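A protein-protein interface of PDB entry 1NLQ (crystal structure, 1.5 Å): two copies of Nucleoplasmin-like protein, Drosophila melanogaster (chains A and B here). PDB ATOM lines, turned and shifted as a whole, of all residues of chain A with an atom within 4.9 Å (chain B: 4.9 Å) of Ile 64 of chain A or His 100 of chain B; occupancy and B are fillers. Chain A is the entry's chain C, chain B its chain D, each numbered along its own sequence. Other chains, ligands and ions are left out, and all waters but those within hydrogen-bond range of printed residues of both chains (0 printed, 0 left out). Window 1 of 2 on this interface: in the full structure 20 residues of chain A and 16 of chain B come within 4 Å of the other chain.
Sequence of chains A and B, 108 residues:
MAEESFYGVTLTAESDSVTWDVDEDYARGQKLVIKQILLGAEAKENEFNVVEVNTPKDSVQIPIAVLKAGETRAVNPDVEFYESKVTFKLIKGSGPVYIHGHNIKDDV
A ring nitrogen (NE2) of His 100 of chain B lies within hydrogen-bond range of the backbone carbonyl oxygen of Pro 63 of chain A (2.7 Å). The side-chain amide nitrogen of Gln 36 of chain B is in hydrogen-bond range of the backbone carbonyl oxygen of Ile 64 of chain A, at 3.2 Å.
O of Val 75 of chain A lies within hydrogen-bond range of N of Ile 37 of chain A, at 3.0 Å. The backbone carbonyl oxygen of Val 51 of chain A sits at hydrogen-bond distance from the backbone NH of Ile 64 of chain A (2.8 Å). The backbone carbonyl oxygen of Ala 65 of chain A lies within hydrogen-bond range of the backbone NH of Val 51 of chain A, 3.0 Å away. The backbone carbonyl oxygen of Ile 62 of chain A sits at hydrogen-bond distance from the backbone NH of Val 53 of chain A, at 2.8 Å. O of Gln 36 of chain B lies within hydrogen-bond range of N of His 100 of chain B (2.8 Å). N of Tyr 98 of chain B sits at hydrogen-bond distance from O of Leu 38 of chain B.
Ile 62 of chain A touches Gly 8 of chain B (CD1 to C, 3.6 Å). Tyr 98 of chain B touches Pro 63 of chain A. Leu 38 of chain B touches Ile 64 of chain A (CD2 to C, 3.5 Å). Ile 64 of chain A touches His 100 of chain B (CA to CE1, 3.7 Å). N of Ala 65 of chain A touches CD2 of Leu 38 of chain B, at 3.5 Å. CD2 of Leu 38 of chain B touches N of Val 66 of chain A (3.8 Å). Pro 77 of chain A touches Lys 35 of chain B (O to CB, 3.4 Å). Pro 77 of chain A touches Gln 36 of chain B. Val 79 of chain A touches Phe 6 of chain B (CB to CE1, 3.9 Å). CB of His 100 of chain B touches CG1 of Val 79 of chain A (3.9 Å).
His 100 of chain B touches just these residues of chain A: Pro 63 (2.7 Å), Ile 64 (3.7 Å) and Val 79 (3.9 Å). Printed residues of chain B within 4 Å of Val 66 of chain A: Leu 38 (3.8 Å). Of the printed residues of chain A, Leu 38 of chain B touches Ile 64 (3.5 Å), Ala 65 (3.5 Å) and Val 66 (3.8 Å). Of the printed residues of chain B, Ala 65 of chain A touches Leu 38 (3.5 Å). Printed residues of chain A within 4 Å of Gly 8 of chain B: Ile 62. Ile 34 of chain B touches none of the printed residues of chain A. Tyr 7 of chain B touches none of the printed residues of chain A. The nearest residue of chain B that does not touch Ile 64 of chain A is Phe 6 of chain B (4.3 Å).
Of the 13 printed residues of chain B, 7 touch a printed residue of chain A. Printed residues of chain B that touch a printed residue of chain A: Phe 6, Gly 8, Lys 35, Gln 36, Leu 38, Tyr 98 and His 100. Printed residues of chain A that touch a printed residue of chain B: Ile 62, Pro 63, Ile 64, Ala 65, Val 66, Val 75, Pro 77 and Val 79. Hydrophobic or aromatic side chains of chain A within 4 Å of the printed part of chain B: Ile 62, Pro 63, Ile 64, Val 66, Val 75, Pro 77 and Val 79. Among the printed residues, no Asp or Glu carboxylate lies within 4 Å of a Lys or Arg side-chain nitrogen of the other chain.
No position is printed for both chains.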
ATOM      1  N   ILE A  37     -14.194 -35.226 -11.743  1.00  0.00           N
ATOM      2  CA  ILE A  37     -15.531 -35.579 -11.290  1.00  0.00           C
ATOM      3  C   ILE A  37     -16.149 -36.096 -12.589  1.00  0.00           C
ATOM      4  O   ILE A  37     -16.272 -35.365 -13.572  1.00  0.00           O
ATOM      5  CB  ILE A  37     -16.277 -34.369 -10.704  1.00  0.00           C
ATOM      6  CG1 ILE A  37     -15.519 -33.866  -9.467  1.00  0.00           C
ATOM      7  CG2 ILE A  37     -17.685 -34.785 -10.282  1.00  0.00           C
ATOM      8  CD1 ILE A  37     -16.086 -32.598  -8.845  1.00  0.00           C
ATOM      9  N   VAL A  51     -22.621 -31.485  -8.243  1.00  0.00           N
ATOM     10  CA  VAL A  51     -21.917 -31.820  -7.015  1.00  0.00           C
ATOM     11  C   VAL A  51     -21.501 -30.518  -6.334  1.00  0.00           C
ATOM     12  O   VAL A  51     -20.811 -29.686  -6.919  1.00  0.00           O
ATOM     13  CB  VAL A  51     -20.658 -32.652  -7.295  1.00  0.00           C
ATOM     14  CG1 VAL A  51     -19.947 -32.969  -5.984  1.00  0.00           C
ATOM     15  CG2 VAL A  51     -21.033 -33.929  -8.011  1.00  0.00           C
ATOM     16  N   GLU A  52     -21.943 -30.348  -5.093  1.00  0.00           N
ATOM     17  CA  GLU A  52     -21.635 -29.159  -4.315  1.00  0.00           C
ATOM     18  C   GLU A  52     -20.581 -29.504  -3.282  1.00  0.00           C
ATOM     19  O   GLU A  52     -20.635 -30.570  -2.676  1.00  0.00           O
ATOM     20  CB  GLU A  52     -22.897 -28.667  -3.596  1.00  0.00           C
ATOM     21  CG  GLU A  52     -22.654 -27.612  -2.520  1.00  0.00           C
ATOM     22  CD  GLU A  52     -23.887 -27.353  -1.654  1.00  0.00           C
ATOM     23  OE1 GLU A  52     -24.792 -26.624  -2.107  1.00  0.00           O
ATOM     24  OE2 GLU A  52     -23.943 -27.888  -0.525  1.00  0.00           O
ATOM     25  N   VAL A  53     -19.610 -28.620  -3.096  1.00  0.00           N
ATOM     26  CA  VAL A  53     -18.591 -28.858  -2.085  1.00  0.00           C
ATOM     27  C   VAL A  53     -18.807 -27.864  -0.953  1.00  0.00           C
ATOM     28  O   VAL A  53     -19.286 -26.752  -1.169  1.00  0.00           O
ATOM     29  CB  VAL A  53     -17.158 -28.665  -2.627  1.00  0.00           C
ATOM     30  CG1 VAL A  53     -16.939 -27.219  -3.035  1.00  0.00           C
ATOM     31  CG2 VAL A  53     -16.145 -29.067  -1.563  1.00  0.00           C
ATOM     32  N   ILE A  62     -20.441 -24.348  -2.549  1.00  0.00           N
ATOM     33  CA  ILE A  62     -20.616 -24.025  -3.961  1.00  0.00           C
ATOM     34  C   ILE A  62     -20.507 -25.234  -4.894  1.00  0.00           C
ATOM     35  O   ILE A  62     -19.816 -26.206  -4.585  1.00  0.00           O
ATOM     36  CB  ILE A  62     -19.534 -22.986  -4.360  1.00  0.00           C
ATOM     37  CG1 ILE A  62     -19.780 -22.423  -5.758  1.00  0.00           C
ATOM     38  CG2 ILE A  62     -18.160 -23.640  -4.304  1.00  0.00           C
ATOM     39  CD1 ILE A  62     -18.830 -21.280  -6.104  1.00  0.00           C
ATOM     40  N   PRO A  63     -21.201 -25.197  -6.045  1.00  0.00           N
ATOM     41  CA  PRO A  63     -21.080 -26.354  -6.941  1.00  0.00           C
ATOM     42  C   PRO A  63     -19.677 -26.406  -7.558  1.00  0.00           C
ATOM     43  O   PRO A  63     -19.111 -25.367  -7.919  1.00  0.00           O
ATOM     44  CB  PRO A  63     -22.144 -26.087  -8.006  1.00  0.00           C
ATOM     45  CG  PRO A  63     -23.155 -25.225  -7.288  1.00  0.00           C
ATOM     46  CD  PRO A  63     -22.270 -24.291  -6.504  1.00  0.00           C
ATOM     47  N   ILE A  64     -19.110 -27.603  -7.663  1.00  0.00           N
ATOM     48  CA  ILE A  64     -17.796 -27.737  -8.279  1.00  0.00           C
ATOM     49  C   ILE A  64     -17.875 -28.610  -9.515  1.00  0.00           C
ATOM     50  O   ILE A  64     -16.885 -28.823 -10.200  1.00  0.00           O
ATOM     51  CB  ILE A  64     -16.729 -28.301  -7.309  1.00  0.00           C
ATOM     52  CG1 ILE A  64     -17.214 -29.597  -6.662  1.00  0.00           C
ATOM     53  CG2 ILE A  64     -16.367 -27.222  -6.280  1.00  0.00           C
ATOM     54  CD1 ILE A  64     -16.140 -30.259  -5.843  1.00  0.00           C
ATOM     55  N   ALA A  65     -19.067 -29.117  -9.795  1.00  0.00           N
ATOM     56  CA  ALA A  65     -19.273 -29.931 -10.978  1.00  0.00           C
ATOM     57  C   ALA A  65     -20.723 -29.859 -11.408  1.00  0.00           C
ATOM     58  O   ALA A  65     -21.628 -29.948 -10.582  1.00  0.00           O
ATOM     59  CB  ALA A  65     -18.895 -31.384 -10.713  1.00  0.00           C
ATOM     60  N   VAL A  66     -20.920 -29.654 -12.703  1.00  0.00           N
ATOM     61  CA  VAL A  66     -22.249 -29.636 -13.308  1.00  0.00           C
ATOM     62  C   VAL A  66     -22.070 -30.561 -14.500  1.00  0.00           C
ATOM     63  O   VAL A  66     -21.336 -30.247 -15.446  1.00  0.00           O
ATOM     64  CB  VAL A  66     -22.664 -28.235 -13.786  1.00  0.00           C
ATOM     65  CG1 VAL A  66     -24.003 -28.319 -14.519  1.00  0.00           C
ATOM     66  CG2 VAL A  66     -22.804 -27.304 -12.589  1.00  0.00           C
ATOM     67  N   VAL A  75     -15.574 -33.192 -15.590  1.00  0.00           N
ATOM     68  CA  VAL A  75     -14.919 -31.915 -15.352  1.00  0.00           C
ATOM     69  C   VAL A  75     -13.629 -32.249 -14.615  1.00  0.00           C
ATOM     70  O   VAL A  75     -13.512 -33.303 -13.981  1.00  0.00           O
ATOM     71  CB  VAL A  75     -15.769 -30.912 -14.503  1.00  0.00           C
ATOM     72  CG1 VAL A  75     -16.960 -30.428 -15.313  1.00  0.00           C
ATOM     73  CG2 VAL A  75     -16.202 -31.541 -13.183  1.00  0.00           C
ATOM     74  N   PRO A  77     -11.689 -30.211 -12.066  1.00  0.00           N
ATOM     75  CA  PRO A  77     -11.508 -29.053 -11.182  1.00  0.00           C
ATOM     76  C   PRO A  77     -10.053 -28.726 -10.826  1.00  0.00           C
ATOM     77  O   PRO A  77      -9.632 -27.563 -10.874  1.00  0.00           O
ATOM     78  CB  PRO A  77     -12.326 -29.426  -9.952  1.00  0.00           C
ATOM     79  CG  PRO A  77     -13.399 -30.350 -10.515  1.00  0.00           C
ATOM     80  CD  PRO A  77     -12.606 -31.199 -11.468  1.00  0.00           C
ATOM     81  N   VAL A  79      -8.772 -28.674  -8.028  1.00  0.00           N
ATOM     82  CA  VAL A  79      -8.817 -27.768  -6.886  1.00  0.00           C
ATOM     83  C   VAL A  79      -8.302 -28.503  -5.654  1.00  0.00           C
ATOM     84  O   VAL A  79      -8.259 -29.735  -5.625  1.00  0.00           O
ATOM     85  CB  VAL A  79     -10.259 -27.236  -6.622  1.00  0.00           C
ATOM     86  CG1 VAL A  79     -10.702 -26.325  -7.771  1.00  0.00           C
ATOM     87  CG2 VAL A  79     -11.226 -28.389  -6.468  1.00  0.00           C
ATOM     88  N   PHE A  88     -18.822 -33.399   0.044  1.00  0.00           N
ATOM     89  CA  PHE A  88     -19.299 -33.322  -1.331  1.00  0.00           C
ATOM     90  C   PHE A  88     -20.701 -33.884  -1.332  1.00  0.00           C
ATOM     91  O   PHE A  88     -20.952 -34.937  -0.748  1.00  0.00           O
ATOM     92  CB  PHE A  88     -18.424 -34.156  -2.279  1.00  0.00           C
ATOM     93  CG  PHE A  88     -16.977 -33.768  -2.271  1.00  0.00           C
ATOM     94  CD1 PHE A  88     -16.053 -34.481  -1.511  1.00  0.00           C
ATOM     95  CD2 PHE A  88     -16.536 -32.676  -3.005  1.00  0.00           C
ATOM     96  CE1 PHE A  88     -14.705 -34.106  -1.484  1.00  0.00           C
ATOM     97  CE2 PHE A  88     -15.196 -32.291  -2.984  1.00  0.00           C
ATOM     98  CZ  PHE A  88     -14.280 -33.010  -2.221  1.00  0.00           C
ATOM     99  N   PHE B   6      -9.149 -22.390  -0.233  1.00  0.00           N
ATOM    100  CA  PHE B   6      -9.963 -22.670  -1.400  1.00  0.00           C
ATOM    101  C   PHE B   6     -10.727 -21.412  -1.767  1.00  0.00           C
ATOM    102  O   PHE B   6     -11.222 -20.702  -0.892  1.00  0.00           O
ATOM    103  CB  PHE B   6     -10.957 -23.791  -1.099  1.00  0.00           C
ATOM    104  CG  PHE B   6     -11.926 -24.044  -2.211  1.00  0.00           C
ATOM    105  CD1 PHE B   6     -11.501 -24.638  -3.393  1.00  0.00           C
ATOM    106  CD2 PHE B   6     -13.261 -23.679  -2.086  1.00  0.00           C
ATOM    107  CE1 PHE B   6     -12.400 -24.866  -4.433  1.00  0.00           C
ATOM    108  CE2 PHE B   6     -14.160 -23.905  -3.120  1.00  0.00           C
ATOM    109  CZ  PHE B   6     -13.729 -24.498  -4.290  1.00  0.00           C
ATOM    110  N   TYR B   7     -10.817 -21.138  -3.064  1.00  0.00           N
ATOM    111  CA  TYR B   7     -11.527 -19.965  -3.553  1.00  0.00           C
ATOM    112  C   TYR B   7     -12.707 -20.454  -4.377  1.00  0.00           C
ATOM    113  O   TYR B   7     -12.528 -21.212  -5.325  1.00  0.00           O
ATOM    114  CB  TYR B   7     -10.608 -19.117  -4.431  1.00  0.00           C
ATOM    115  CG  TYR B   7     -11.194 -17.776  -4.821  1.00  0.00           C
ATOM    116  CD1 TYR B   7     -11.385 -16.772  -3.872  1.00  0.00           C
ATOM    117  CD2 TYR B   7     -11.559 -17.509  -6.140  1.00  0.00           C
ATOM    118  CE1 TYR B   7     -11.916 -15.543  -4.226  1.00  0.00           C
ATOM    119  CE2 TYR B   7     -12.100 -16.278  -6.505  1.00  0.00           C
ATOM    120  CZ  TYR B   7     -12.274 -15.302  -5.541  1.00  0.00           C
ATOM    121  OH  TYR B   7     -12.811 -14.092  -5.891  1.00  0.00           O
ATOM    122  N   GLY B   8     -13.909 -20.032  -3.999  1.00  0.00           N
ATOM    123  CA  GLY B   8     -15.099 -20.432  -4.727  1.00  0.00           C
ATOM    124  C   GLY B   8     -16.119 -19.315  -4.652  1.00  0.00           C
ATOM    125  O   GLY B   8     -16.682 -19.063  -3.591  1.00  0.00           O
ATOM    126  N   VAL B  33      -4.950 -18.264  -7.783  1.00  0.00           N
ATOM    127  CA  VAL B  33      -4.873 -19.170  -8.920  1.00  0.00           C
ATOM    128  C   VAL B  33      -6.292 -19.565  -9.308  1.00  0.00           C
ATOM    129  O   VAL B  33      -7.038 -20.065  -8.476  1.00  0.00           O
ATOM    130  CB  VAL B  33      -4.089 -20.453  -8.573  1.00  0.00           C
ATOM    131  CG1 VAL B  33      -3.982 -21.348  -9.794  1.00  0.00           C
ATOM    132  CG2 VAL B  33      -2.689 -20.100  -8.064  1.00  0.00           C
ATOM    133  N   ILE B  34      -6.668 -19.325 -10.556  1.00  0.00           N
ATOM    134  CA  ILE B  34      -8.004 -19.681 -11.013  1.00  0.00           C
ATOM    135  C   ILE B  34      -7.921 -20.973 -11.812  1.00  0.00           C
ATOM    136  O   ILE B  34      -7.376 -21.018 -12.914  1.00  0.00           O
ATOM    137  CB  ILE B  34      -8.627 -18.557 -11.867  1.00  0.00           C
ATOM    138  CG1 ILE B  34      -8.755 -17.280 -11.026  1.00  0.00           C
ATOM    139  CG2 ILE B  34      -9.995 -18.993 -12.388  1.00  0.00           C
ATOM    140  CD1 ILE B  34      -9.522 -17.466  -9.721  1.00  0.00           C
ATOM    141  N   LYS B  35      -8.479 -22.030 -11.239  1.00  0.00           N
ATOM    142  CA  LYS B  35      -8.442 -23.355 -11.844  1.00  0.00           C
ATOM    143  C   LYS B  35      -9.607 -23.728 -12.753  1.00  0.00           C
ATOM    144  O   LYS B  35      -9.418 -24.410 -13.761  1.00  0.00           O
ATOM    145  CB  LYS B  35      -8.337 -24.408 -10.732  1.00  0.00           C
ATOM    146  CG  LYS B  35      -6.997 -24.444 -10.023  1.00  0.00           C
ATOM    147  CD  LYS B  35      -5.929 -24.937 -10.983  1.00  0.00           C
ATOM    148  CE  LYS B  35      -4.585 -25.145 -10.297  1.00  0.00           C
ATOM    149  NZ  LYS B  35      -3.603 -25.728 -11.256  1.00  0.00           N
ATOM    150  N   GLN B  36     -10.809 -23.302 -12.389  1.00  0.00           N
ATOM    151  CA  GLN B  36     -11.987 -23.644 -13.175  1.00  0.00           C
ATOM    152  C   GLN B  36     -13.078 -22.584 -13.108  1.00  0.00           C
ATOM    153  O   GLN B  36     -13.250 -21.916 -12.097  1.00  0.00           O
ATOM    154  CB  GLN B  36     -12.548 -24.989 -12.680  1.00  0.00           C
ATOM    155  CG  GLN B  36     -13.822 -25.482 -13.377  1.00  0.00           C
ATOM    156  CD  GLN B  36     -14.348 -26.797 -12.790  1.00  0.00           C
ATOM    157  OE1 GLN B  36     -14.259 -27.849 -13.420  1.00  0.00           O
ATOM    158  NE2 GLN B  36     -14.889 -26.734 -11.577  1.00  0.00           N
ATOM    159  N   LEU B  38     -17.021 -22.598 -14.088  1.00  0.00           N
ATOM    160  CA  LEU B  38     -18.094 -23.516 -14.431  1.00  0.00           C
ATOM    161  C   LEU B  38     -19.478 -22.891 -14.560  1.00  0.00           C
ATOM    162  O   LEU B  38     -19.885 -22.075 -13.738  1.00  0.00           O
ATOM    163  CB  LEU B  38     -18.111 -24.611 -13.365  1.00  0.00           C
ATOM    164  CG  LEU B  38     -19.163 -25.719 -13.354  1.00  0.00           C
ATOM    165  CD1 LEU B  38     -18.917 -26.717 -14.480  1.00  0.00           C
ATOM    166  CD2 LEU B  38     -19.088 -26.415 -11.991  1.00  0.00           C
ATOM    167  N   TYR B  98     -19.642 -20.220 -11.679  1.00  0.00           N
ATOM    168  CA  TYR B  98     -18.829 -20.414 -10.490  1.00  0.00           C
ATOM    169  C   TYR B  98     -17.359 -20.297 -10.854  1.00  0.00           C
ATOM    170  O   TYR B  98     -16.936 -20.776 -11.903  1.00  0.00           O
ATOM    171  CB  TYR B  98     -19.103 -21.792  -9.882  1.00  0.00           C
ATOM    172  CG  TYR B  98     -20.570 -22.140  -9.816  1.00  0.00           C
ATOM    173  CD1 TYR B  98     -21.109 -23.140 -10.633  1.00  0.00           C
ATOM    174  CD2 TYR B  98     -21.430 -21.458  -8.955  1.00  0.00           C
ATOM    175  CE1 TYR B  98     -22.462 -23.446 -10.592  1.00  0.00           C
ATOM    176  CE2 TYR B  98     -22.784 -21.760  -8.908  1.00  0.00           C
ATOM    177  CZ  TYR B  98     -23.291 -22.751  -9.727  1.00  0.00           C
ATOM    178  OH  TYR B  98     -24.626 -23.046  -9.683  1.00  0.00           O
ATOM    179  N   ILE B  99     -16.588 -19.637  -9.993  1.00  0.00           N
ATOM    180  CA  ILE B  99     -15.149 -19.491 -10.204  1.00  0.00           C
ATOM    181  C   ILE B  99     -14.436 -20.232  -9.068  1.00  0.00           C
ATOM    182  O   ILE B  99     -14.676 -19.956  -7.891  1.00  0.00           O
ATOM    183  CB  ILE B  99     -14.731 -18.008 -10.198  1.00  0.00           C
ATOM    184  CG1 ILE B  99     -15.435 -17.267 -11.344  1.00  0.00           C
ATOM    185  CG2 ILE B  99     -13.214 -17.890 -10.382  1.00  0.00           C
ATOM    186  CD1 ILE B  99     -15.209 -15.761 -11.334  1.00  0.00           C
ATOM    187  N   HIS B 100     -13.579 -21.183  -9.425  1.00  0.00           N
ATOM    188  CA  HIS B 100     -12.857 -21.980  -8.438  1.00  0.00           C
ATOM    189  C   HIS B 100     -11.350 -21.860  -8.566  1.00  0.00           C
ATOM    190  O   HIS B 100     -10.800 -21.784  -9.666  1.00  0.00           O
ATOM    191  CB  HIS B 100     -13.194 -23.466  -8.577  1.00  0.00           C
ATOM    192  CG  HIS B 100     -14.658 -23.764  -8.621  1.00  0.00           C
ATOM    193  ND1 HIS B 100     -15.261 -24.350  -9.713  1.00  0.00           N
ATOM    194  CD2 HIS B 100     -15.636 -23.580  -7.703  1.00  0.00           C
ATOM    195  CE1 HIS B 100     -16.549 -24.517  -9.464  1.00  0.00           C
ATOM    196  NE2 HIS B 100     -16.801 -24.058  -8.251  1.00  0.00           N
ATOM    197  N   GLY B 101     -10.684 -21.879  -7.423  1.00  0.00           N
ATOM    198  CA  GLY B 101      -9.242 -21.796  -7.424  1.00  0.00           C
ATOM    199  C   GLY B 101      -8.732 -21.816  -6.005  1.00  0.00           C
ATOM    200  O   GLY B 101      -9.305 -22.460  -5.125  1.00  0.00           O
ATOM    201  N   HIS B 102      -7.632 -21.120  -5.779  1.00  0.00           N
ATOM    202  CA  HIS B 102      -7.088 -21.044  -4.440  1.00  0.00           C
ATOM    203  C   HIS B 102      -6.157 -19.869  -4.309  1.00  0.00           C
ATOM    204  O   HIS B 102      -5.567 -19.410  -5.287  1.00  0.00           O
ATOM    205  CB  HIS B 102      -6.350 -22.331  -4.071  1.00  0.00           C
ATOM    206  CG  HIS B 102      -5.289 -22.727  -5.051  1.00  0.00           C
ATOM    207  ND1 HIS B 102      -5.481 -23.714  -5.993  1.00  0.00           N
ATOM    208  CD2 HIS B 102      -4.018 -22.293  -5.217  1.00  0.00           C
ATOM    209  CE1 HIS B 102      -4.376 -23.873  -6.697  1.00  0.00           C
ATOM    210  NE2 HIS B 102      -3.470 -23.023  -6.246  1.00  0.00           N
